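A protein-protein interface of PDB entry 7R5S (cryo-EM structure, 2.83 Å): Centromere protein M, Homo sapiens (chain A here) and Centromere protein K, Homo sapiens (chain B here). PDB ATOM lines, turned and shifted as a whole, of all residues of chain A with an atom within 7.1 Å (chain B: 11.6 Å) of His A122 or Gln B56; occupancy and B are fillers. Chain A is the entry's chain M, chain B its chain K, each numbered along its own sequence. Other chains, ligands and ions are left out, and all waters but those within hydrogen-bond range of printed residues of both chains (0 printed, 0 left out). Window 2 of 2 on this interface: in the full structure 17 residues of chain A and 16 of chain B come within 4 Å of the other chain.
OD1 of Asn B54 is in hydrogen-bond range of N of Thr B51, 3.2 Å away.
OG1 of Thr A123 is in hydrogen-bond range of O of Lys A119, at 2.7 Å.
OE1 of Gln A125 lies close to O of His A122.
OG of Ser A126 lies within hydrogen-bond range of O of Tyr A124 (3.3 Å).
Among the printed residues, pairs that only touch across the chains: His A122 with Gln B56 (3.6 Å), Thr A123 with Gln B56 (3.97 Å), Tyr A124 with Thr B51 (3.9 Å), Tyr A124 with Leu B59 (3.3 Å) and Gln A125 with Gln B56 (3.5 Å).
Leu A120 touches none of the printed residues of chain B.
No residue of chain B comes within 4 Å of Ala A121.
His A122 touches just one residue of chain B: Gln B56.
Of the printed residues of chain B, Tyr A124 touches Thr B51 and Leu B59.
No residue of chain B comes within 4 Å of Ser A126.
Of the printed residues of chain A, Thr B51 touches Tyr A124.
Printed residues of chain A within 4 Å of Gln B56: His A122, Thr A123 and Gln A125.
Printed residues of chain A within 4 Å of Leu B59: Tyr A124.
The nearest residue of chain B that does not touch His A122 is Leu B59 (7.0 Å).
Hydrophobic or aromatic side chains of chain A that line the printed part of chain B: His A122 and Tyr A124.
Along chain A the printed residues that touch a printed residue of chain B span positions 122 to 125.
Of the 17 printed residues of chain B, 3 touch a printed residue of chain A.
Hydrophobic or aromatic side chains of chain B that line the printed part of chain A: Leu B59.
Among the printed residues, 5 pairs touch across the chains.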
ATOM      1  N   PHE A  99      21.639  -0.302  12.864  1.00  0.00           N
ATOM      2  CA  PHE A  99      21.597  -1.067  11.625  1.00  0.00           C
ATOM      3  C   PHE A  99      22.831  -0.737  10.800  1.00  0.00           C
ATOM      4  O   PHE A  99      23.199   0.435  10.671  1.00  0.00           O
ATOM      5  CB  PHE A  99      20.329  -0.760  10.823  1.00  0.00           C
ATOM      6  CG  PHE A  99      19.062  -1.233  11.478  1.00  0.00           C
ATOM      7  CD1 PHE A  99      18.621  -2.533  11.304  1.00  0.00           C
ATOM      8  CD2 PHE A  99      18.310  -0.375  12.262  1.00  0.00           C
ATOM      9  CE1 PHE A  99      17.456  -2.971  11.904  1.00  0.00           C
ATOM     10  CE2 PHE A  99      17.143  -0.807  12.863  1.00  0.00           C
ATOM     11  CZ  PHE A  99      16.716  -2.106  12.684  1.00  0.00           C
ATOM     12  N   THR A 116      14.331   0.228   0.883  1.00  0.00           N
ATOM     13  CA  THR A 116      13.832  -0.778   1.816  1.00  0.00           C
ATOM     14  C   THR A 116      14.508  -0.653   3.175  1.00  0.00           C
ATOM     15  O   THR A 116      13.837  -0.581   4.211  1.00  0.00           O
ATOM     16  CB  THR A 116      14.042  -2.178   1.237  1.00  0.00           C
ATOM     17  OG1 THR A 116      13.333  -2.296  -0.003  1.00  0.00           O
ATOM     18  CG2 THR A 116      13.537  -3.236   2.204  1.00  0.00           C
ATOM     19  N   VAL A 117      15.844  -0.617   3.194  1.00  0.00           N
ATOM     20  CA  VAL A 117      16.548  -0.520   4.469  1.00  0.00           C
ATOM     21  C   VAL A 117      16.361   0.860   5.089  1.00  0.00           C
ATOM     22  O   VAL A 117      16.333   0.992   6.318  1.00  0.00           O
ATOM     23  CB  VAL A 117      18.038  -0.872   4.300  1.00  0.00           C
ATOM     24  CG1 VAL A 117      18.196  -2.343   3.950  1.00  0.00           C
ATOM     25  CG2 VAL A 117      18.686   0.000   3.242  1.00  0.00           C
ATOM     26  N   VAL A 118      16.205   1.902   4.267  1.00  0.00           N
ATOM     27  CA  VAL A 118      15.934   3.232   4.810  1.00  0.00           C
ATOM     28  C   VAL A 118      14.604   3.239   5.557  1.00  0.00           C
ATOM     29  O   VAL A 118      14.504   3.735   6.686  1.00  0.00           O
ATOM     30  CB  VAL A 118      15.962   4.287   3.690  1.00  0.00           C
ATOM     31  CG1 VAL A 118      15.257   5.557   4.137  1.00  0.00           C
ATOM     32  CG2 VAL A 118      17.394   4.593   3.290  1.00  0.00           C
ATOM     33  N   LYS A 119      13.563   2.671   4.941  1.00  0.00           N
ATOM     34  CA  LYS A 119      12.259   2.606   5.591  1.00  0.00           C
ATOM     35  C   LYS A 119      12.294   1.699   6.814  1.00  0.00           C
ATOM     36  O   LYS A 119      11.634   1.982   7.822  1.00  0.00           O
ATOM     37  CB  LYS A 119      11.204   2.128   4.594  1.00  0.00           C
ATOM     38  CG  LYS A 119       9.793   2.072   5.152  1.00  0.00           C
ATOM     39  CD  LYS A 119       8.812   1.558   4.112  1.00  0.00           C
ATOM     40  CE  LYS A 119       7.396   1.512   4.662  1.00  0.00           C
ATOM     41  NZ  LYS A 119       6.908   2.863   5.052  1.00  0.00           N
ATOM     42  N   LEU A 120      13.059   0.607   6.750  1.00  0.00           N
ATOM     43  CA  LEU A 120      13.170  -0.285   7.900  1.00  0.00           C
ATOM     44  C   LEU A 120      13.834   0.414   9.078  1.00  0.00           C
ATOM     45  O   LEU A 120      13.422   0.234  10.230  1.00  0.00           O
ATOM     46  CB  LEU A 120      13.948  -1.544   7.513  1.00  0.00           C
ATOM     47  CG  LEU A 120      14.186  -2.565   8.628  1.00  0.00           C
ATOM     48  CD1 LEU A 120      12.867  -3.104   9.155  1.00  0.00           C
ATOM     49  CD2 LEU A 120      15.074  -3.696   8.137  1.00  0.00           C
ATOM     50  N   ALA A 121      14.867   1.216   8.811  1.00  0.00           N
ATOM     51  CA  ALA A 121      15.529   1.946   9.887  1.00  0.00           C
ATOM     52  C   ALA A 121      14.644   3.066  10.420  1.00  0.00           C
ATOM     53  O   ALA A 121      14.646   3.342  11.625  1.00  0.00           O
ATOM     54  CB  ALA A 121      16.866   2.503   9.399  1.00  0.00           C
ATOM     55  N   HIS A 122      13.882   3.721   9.541  1.00  0.00           N
ATOM     56  CA  HIS A 122      13.010   4.801   9.990  1.00  0.00           C
ATOM     57  C   HIS A 122      11.827   4.278  10.795  1.00  0.00           C
ATOM     58  O   HIS A 122      11.330   4.977  11.685  1.00  0.00           O
ATOM     59  CB  HIS A 122      12.516   5.611   8.792  1.00  0.00           C
ATOM     60  CG  HIS A 122      11.499   6.651   9.144  1.00  0.00           C
ATOM     61  ND1 HIS A 122      10.146   6.455   8.976  1.00  0.00           N
ATOM     62  CD2 HIS A 122      11.639   7.896   9.658  1.00  0.00           C
ATOM     63  CE1 HIS A 122       9.495   7.535   9.371  1.00  0.00           C
ATOM     64  NE2 HIS A 122      10.377   8.424   9.789  1.00  0.00           N
ATOM     65  N   THR A 123      11.365   3.060  10.502  1.00  0.00           N
ATOM     66  CA  THR A 123      10.204   2.521  11.203  1.00  0.00           C
ATOM     67  C   THR A 123      10.511   2.260  12.674  1.00  0.00           C
ATOM     68  O   THR A 123       9.695   2.575  13.547  1.00  0.00           O
ATOM     69  CB  THR A 123       9.730   1.237  10.520  1.00  0.00           C
ATOM     70  OG1 THR A 123       9.385   1.518   9.159  1.00  0.00           O
ATOM     71  CG2 THR A 123       8.516   0.666  11.236  1.00  0.00           C
ATOM     72  N   TYR A 124      11.678   1.694  12.968  1.00  0.00           N
ATOM     73  CA  TYR A 124      12.048   1.335  14.329  1.00  0.00           C
ATOM     74  C   TYR A 124      12.825   2.432  15.047  1.00  0.00           C
ATOM     75  O   TYR A 124      13.307   2.200  16.160  1.00  0.00           O
ATOM     76  CB  TYR A 124      12.859   0.037  14.326  1.00  0.00           C
ATOM     77  CG  TYR A 124      12.020  -1.199  14.096  1.00  0.00           C
ATOM     78  CD1 TYR A 124      11.731  -1.636  12.811  1.00  0.00           C
ATOM     79  CD2 TYR A 124      11.512  -1.926  15.165  1.00  0.00           C
ATOM     80  CE1 TYR A 124      10.962  -2.764  12.596  1.00  0.00           C
ATOM     81  CE2 TYR A 124      10.742  -3.054  14.960  1.00  0.00           C
ATOM     82  CZ  TYR A 124      10.471  -3.469  13.674  1.00  0.00           C
ATOM     83  OH  TYR A 124       9.705  -4.593  13.466  1.00  0.00           O
ATOM     84  N   GLN A 125      12.956   3.612  14.438  1.00  0.00           N
ATOM     85  CA  GLN A 125      13.608   4.769  15.054  1.00  0.00           C
ATOM     86  C   GLN A 125      15.029   4.428  15.510  1.00  0.00           C
ATOM     87  O   GLN A 125      15.363   4.478  16.694  1.00  0.00           O
ATOM     88  CB  GLN A 125      12.770   5.309  16.218  1.00  0.00           C
ATOM     89  CG  GLN A 125      11.331   5.643  15.853  1.00  0.00           C
ATOM     90  CD  GLN A 125      11.216   6.902  15.018  1.00  0.00           C
ATOM     91  OE1 GLN A 125      10.324   7.023  14.178  1.00  0.00           O
ATOM     92  NE2 GLN A 125      12.116   7.849  15.247  1.00  0.00           N
ATOM     93  N   SER A 126      15.866   4.077  14.539  1.00  0.00           N
ATOM     94  CA  SER A 126      17.239   3.681  14.801  1.00  0.00           C
ATOM     95  C   SER A 126      18.141   4.211  13.697  1.00  0.00           C
ATOM     96  O   SER A 126      17.689   4.405  12.563  1.00  0.00           O
ATOM     97  CB  SER A 126      17.374   2.153  14.891  1.00  0.00           C
ATOM     98  OG  SER A 126      16.522   1.626  15.892  1.00  0.00           O
ATOM     99  N   LEU A 128      21.181   4.342  10.806  1.00  0.00           N
ATOM    100  CA  LEU A 128      21.565   3.470   9.702  1.00  0.00           C
ATOM    101  C   LEU A 128      22.971   3.838   9.259  1.00  0.00           C
ATOM    102  O   LEU A 128      23.238   5.000   8.936  1.00  0.00           O
ATOM    103  CB  LEU A 128      20.583   3.592   8.533  1.00  0.00           C
ATOM    104  CG  LEU A 128      20.889   2.750   7.294  1.00  0.00           C
ATOM    105  CD1 LEU A 128      20.844   1.268   7.626  1.00  0.00           C
ATOM    106  CD2 LEU A 128      19.922   3.080   6.168  1.00  0.00           C
ATOM    107  N   SER A 171      17.190  12.091  12.606  1.00  0.00           N
ATOM    108  CA  SER A 171      17.124  12.634  11.259  1.00  0.00           C
ATOM    109  C   SER A 171      15.958  13.606  11.132  1.00  0.00           C
ATOM    110  O   SER A 171      14.931  13.465  11.800  1.00  0.00           O
ATOM    111  CB  SER A 171      16.982  11.512  10.229  1.00  0.00           C
ATOM    112  OG  SER A 171      18.118  10.665  10.238  1.00  0.00           O
ATOM    113  N   SER A 172      16.130  14.601  10.261  1.00  0.00           N
ATOM    114  CA  SER A 172      15.086  15.602  10.065  1.00  0.00           C
ATOM    115  C   SER A 172      13.893  15.013   9.322  1.00  0.00           C
ATOM    116  O   SER A 172      12.755  15.074   9.804  1.00  0.00           O
ATOM    117  CB  SER A 172      15.649  16.808   9.314  1.00  0.00           C
ATOM    118  OG  SER A 172      16.558  17.534  10.123  1.00  0.00           O
ATOM    119  N   GLU A 173      14.130  14.439   8.147  1.00  0.00           N
ATOM    120  CA  GLU A 173      13.064  13.824   7.366  1.00  0.00           C
ATOM    121  C   GLU A 173      13.220  12.308   7.323  1.00  0.00           C
ATOM    122  O   GLU A 173      14.044  11.780   6.576  1.00  0.00           O
ATOM    123  CB  GLU A 173      13.041  14.391   5.944  1.00  0.00           C
ATOM    124  CG  GLU A 173      12.048  15.527   5.737  1.00  0.00           C
ATOM    125  CD  GLU A 173      12.465  16.808   6.434  1.00  0.00           C
ATOM    126  OE1 GLU A 173      13.668  16.965   6.729  1.00  0.00           O
ATOM    127  OE2 GLU A 173      11.588  17.660   6.687  1.00  0.00           O
ATOM    128  N   THR B  49       6.664  -6.706  23.017  1.00  0.00           N
ATOM    129  CA  THR B  49       7.258  -6.787  21.692  1.00  0.00           C
ATOM    130  C   THR B  49       6.447  -5.966  20.695  1.00  0.00           C
ATOM    131  O   THR B  49       5.245  -5.747  20.863  1.00  0.00           O
ATOM    132  CB  THR B  49       7.349  -8.240  21.221  1.00  0.00           C
ATOM    133  OG1 THR B  49       6.042  -8.826  21.212  1.00  0.00           O
ATOM    134  CG2 THR B  49       8.253  -9.043  22.143  1.00  0.00           C
ATOM    135  N   LEU B  50       7.126  -5.511  19.648  1.00  0.00           N
ATOM    136  CA  LEU B  50       6.527  -4.670  18.624  1.00  0.00           C
ATOM    137  C   LEU B  50       6.409  -5.429  17.310  1.00  0.00           C
ATOM    138  O   LEU B  50       7.002  -6.494  17.117  1.00  0.00           O
ATOM    139  CB  LEU B  50       7.347  -3.391  18.422  1.00  0.00           C
ATOM    140  CG  LEU B  50       7.519  -2.474  19.633  1.00  0.00           C
ATOM    141  CD1 LEU B  50       8.342  -1.255  19.257  1.00  0.00           C
ATOM    142  CD2 LEU B  50       6.167  -2.060  20.190  1.00  0.00           C
ATOM    143  N   THR B  51       5.626  -4.858  16.399  1.00  0.00           N
ATOM    144  CA  THR B  51       5.454  -5.377  15.051  1.00  0.00           C
ATOM    145  C   THR B  51       5.785  -4.274  14.053  1.00  0.00           C
ATOM    146  O   THR B  51       6.210  -3.177  14.425  1.00  0.00           O
ATOM    147  CB  THR B  51       4.029  -5.902  14.828  1.00  0.00           C
ATOM    148  OG1 THR B  51       3.089  -4.840  15.031  1.00  0.00           O
ATOM    149  CG2 THR B  51       3.720  -7.039  15.791  1.00  0.00           C
ATOM    150  N   ASP B  52       5.588  -4.571  12.771  1.00  0.00           N
ATOM    151  CA  ASP B  52       5.871  -3.606  11.717  1.00  0.00           C
ATOM    152  C   ASP B  52       4.812  -2.515  11.615  1.00  0.00           C
ATOM    153  O   ASP B  52       5.070  -1.480  10.994  1.00  0.00           O
ATOM    154  CB  ASP B  52       6.006  -4.336  10.375  1.00  0.00           C
ATOM    155  CG  ASP B  52       6.816  -3.552   9.356  1.00  0.00           C
ATOM    156  OD1 ASP B  52       7.941  -3.987   9.035  1.00  0.00           O
ATOM    157  OD2 ASP B  52       6.326  -2.518   8.857  1.00  0.00           O
ATOM    158  N   SER B  53       3.643  -2.707  12.225  1.00  0.00           N
ATOM    159  CA  SER B  53       2.539  -1.764  12.090  1.00  0.00           C
ATOM    160  C   SER B  53       2.382  -0.827  13.279  1.00  0.00           C
ATOM    161  O   SER B  53       1.957   0.317  13.095  1.00  0.00           O
ATOM    162  CB  SER B  53       1.223  -2.519  11.876  1.00  0.00           C
ATOM    163  OG  SER B  53       1.380  -3.560  10.927  1.00  0.00           O
ATOM    164  N   ASN B  54       2.708  -1.275  14.489  1.00  0.00           N
ATOM    165  CA  ASN B  54       2.503  -0.490  15.700  1.00  0.00           C
ATOM    166  C   ASN B  54       3.815  -0.244  16.435  1.00  0.00           C
ATOM    167  O   ASN B  54       3.901  -0.389  17.656  1.00  0.00           O
ATOM    168  CB  ASN B  54       1.491  -1.170  16.621  1.00  0.00           C
ATOM    169  CG  ASN B  54       1.852  -2.613  16.922  1.00  0.00           C
ATOM    170  OD1 ASN B  54       2.909  -3.100  16.521  1.00  0.00           O
ATOM    171  ND2 ASN B  54       0.972  -3.305  17.633  1.00  0.00           N
ATOM    172  N   ALA B  55       4.857   0.135  15.698  1.00  0.00           N
ATOM    173  CA  ALA B  55       6.167   0.391  16.285  1.00  0.00           C
ATOM    174  C   ALA B  55       6.469   1.873  16.454  1.00  0.00           C
ATOM    175  O   ALA B  55       6.958   2.281  17.512  1.00  0.00           O
ATOM    176  CB  ALA B  55       7.263  -0.255  15.432  1.00  0.00           C
ATOM    177  N   GLN B  56       6.180   2.688  15.438  1.00  0.00           N
ATOM    178  CA  GLN B  56       6.576   4.094  15.471  1.00  0.00           C
ATOM    179  C   GLN B  56       5.854   4.851  16.581  1.00  0.00           C
ATOM    180  O   GLN B  56       6.486   5.552  17.382  1.00  0.00           O
ATOM    181  CB  GLN B  56       6.308   4.736  14.110  1.00  0.00           C
ATOM    182  CG  GLN B  56       6.941   6.104  13.927  1.00  0.00           C
ATOM    183  CD  GLN B  56       6.899   6.572  12.486  1.00  0.00           C
ATOM    184  OE1 GLN B  56       6.505   5.826  11.590  1.00  0.00           O
ATOM    185  NE2 GLN B  56       7.308   7.815  12.256  1.00  0.00           N
ATOM    186  N   LEU B  57       4.527   4.722  16.643  1.00  0.00           N
ATOM    187  CA  LEU B  57       3.759   5.451  17.650  1.00  0.00           C
ATOM    188  C   LEU B  57       4.093   4.974  19.059  1.00  0.00           C
ATOM    189  O   LEU B  57       4.212   5.787  19.986  1.00  0.00           O
ATOM    190  CB  LEU B  57       2.264   5.304  17.370  1.00  0.00           C
ATOM    191  CG  LEU B  57       1.314   6.107  18.259  1.00  0.00           C
ATOM    192  CD1 LEU B  57       1.575   7.598  18.112  1.00  0.00           C
ATOM    193  CD2 LEU B  57      -0.131   5.777  17.925  1.00  0.00           C
ATOM    194  N   SER B  58       4.247   3.661  19.239  1.00  0.00           N
ATOM    195  CA  SER B  58       4.604   3.132  20.552  1.00  0.00           C
ATOM    196  C   SER B  58       5.970   3.642  20.994  1.00  0.00           C
ATOM    197  O   SER B  58       6.152   4.027  22.157  1.00  0.00           O
ATOM    198  CB  SER B  58       4.584   1.604  20.525  1.00  0.00           C
ATOM    199  OG  SER B  58       3.438   1.122  19.849  1.00  0.00           O
ATOM    200  N   LEU B  59       6.940   3.663  20.077  1.00  0.00           N
ATOM    201  CA  LEU B  59       8.264   4.162  20.425  1.00  0.00           C
ATOM    202  C   LEU B  59       8.228   5.653  20.730  1.00  0.00           C
ATOM    203  O   LEU B  59       8.944   6.123  21.620  1.00  0.00           O
ATOM    204  CB  LEU B  59       9.253   3.859  19.300  1.00  0.00           C
ATOM    205  CG  LEU B  59       9.689   2.396  19.198  1.00  0.00           C
ATOM    206  CD1 LEU B  59      10.662   2.200  18.050  1.00  0.00           C
ATOM    207  CD2 LEU B  59      10.300   1.926  20.509  1.00  0.00           C
ATOM    208  N   LEU B  60       7.390   6.413  20.020  1.00  0.00           N
ATOM    209  CA  LEU B  60       7.263   7.838  20.320  1.00  0.00           C
ATOM    210  C   LEU B  60       6.677   8.060  21.711  1.00  0.00           C
ATOM    211  O   LEU B  60       7.151   8.920  22.465  1.00  0.00           O
ATOM    212  CB  LEU B  60       6.405   8.525  19.259  1.00  0.00           C
ATOM    213  CG  LEU B  60       7.041   8.709  17.880  1.00  0.00           C
ATOM    214  CD1 LEU B  60       6.063   9.364  16.920  1.00  0.00           C
ATOM    215  CD2 LEU B  60       8.319   9.524  17.983  1.00  0.00           C
ATOM    216  N   ILE B  61       5.647   7.290  22.069  1.00  0.00           N
ATOM    217  CA  ILE B  61       5.054   7.415  23.400  1.00  0.00           C
ATOM    218  C   ILE B  61       6.072   7.046  24.474  1.00  0.00           C
ATOM    219  O   ILE B  61       6.182   7.721  25.510  1.00  0.00           O
ATOM    220  CB  ILE B  61       3.782   6.553  23.502  1.00  0.00           C
ATOM    221  CG1 ILE B  61       2.720   7.049  22.519  1.00  0.00           C
ATOM    222  CG2 ILE B  61       3.238   6.565  24.921  1.00  0.00           C
ATOM    223  CD1 ILE B  61       2.313   8.489  22.733  1.00  0.00           C
ATOM    224  N   MET B  62       6.831   5.971  24.248  1.00  0.00           N
ATOM    225  CA  MET B  62       7.848   5.572  25.214  1.00  0.00           C
ATOM    226  C   MET B  62       8.933   6.633  25.348  1.00  0.00           C
ATOM    227  O   MET B  62       9.426   6.891  26.453  1.00  0.00           O
ATOM    228  CB  MET B  62       8.457   4.228  24.817  1.00  0.00           C
ATOM    229  CG  MET B  62       7.506   3.055  24.964  1.00  0.00           C
ATOM    230  SD  MET B  62       8.336   1.468  24.766  1.00  0.00           S
ATOM    231  CE  MET B  62       9.512   1.532  26.114  1.00  0.00           C
ATOM    232  N   GLN B  63       9.318   7.261  24.233  1.00  0.00           N
ATOM    233  CA  GLN B  63      10.301   8.336  24.291  1.00  0.00           C
ATOM    234  C   GLN B  63       9.775   9.517  25.094  1.00  0.00           C
ATOM    235  O   GLN B  63      10.512  10.117  25.884  1.00  0.00           O
ATOM    236  CB  GLN B  63      10.680   8.781  22.879  1.00  0.00           C
ATOM    237  CG  GLN B  63      11.582   7.813  22.137  1.00  0.00           C
ATOM    238  CD  GLN B  63      11.799   8.214  20.693  1.00  0.00           C
ATOM    239  OE1 GLN B  63      11.601   9.370  20.321  1.00  0.00           O
ATOM    240  NE2 GLN B  63      12.203   7.256  19.867  1.00  0.00           N
ATOM    241  N   VAL B  64       8.500   9.864  24.903  1.00  0.00           N
ATOM    242  CA  VAL B  64       7.906  10.957  25.671  1.00  0.00           C
ATOM    243  C   VAL B  64       7.946  10.642  27.161  1.00  0.00           C
ATOM    244  O   VAL B  64       8.343  11.479  27.983  1.00  0.00           O
ATOM    245  CB  VAL B  64       6.471  11.234  25.192  1.00  0.00           C
ATOM    246  CG1 VAL B  64       5.743  12.126  26.185  1.00  0.00           C
ATOM    247  CG2 VAL B  64       6.492  11.879  23.824  1.00  0.00           C
ATOM    248  N   LYS B  65       7.540   9.424  27.530  1.00  0.00           N
ATOM    249  CA  LYS B  65       7.530   9.045  28.942  1.00  0.00           C
ATOM    250  C   LYS B  65       8.937   9.072  29.531  1.00  0.00           C
ATOM    251  O   LYS B  65       9.156   9.583  30.638  1.00  0.00           O
ATOM    252  CB  LYS B  65       6.902   7.662  29.108  1.00  0.00           C
ATOM    253  CG  LYS B  65       5.430   7.602  28.742  1.00  0.00           C
ATOM    254  CD  LYS B  65       4.866   6.208  28.961  1.00  0.00           C
ATOM    255  CE  LYS B  65       3.388   6.151  28.620  1.00  0.00           C
ATOM    256  NZ  LYS B  65       2.832   4.781  28.788  1.00  0.00           N
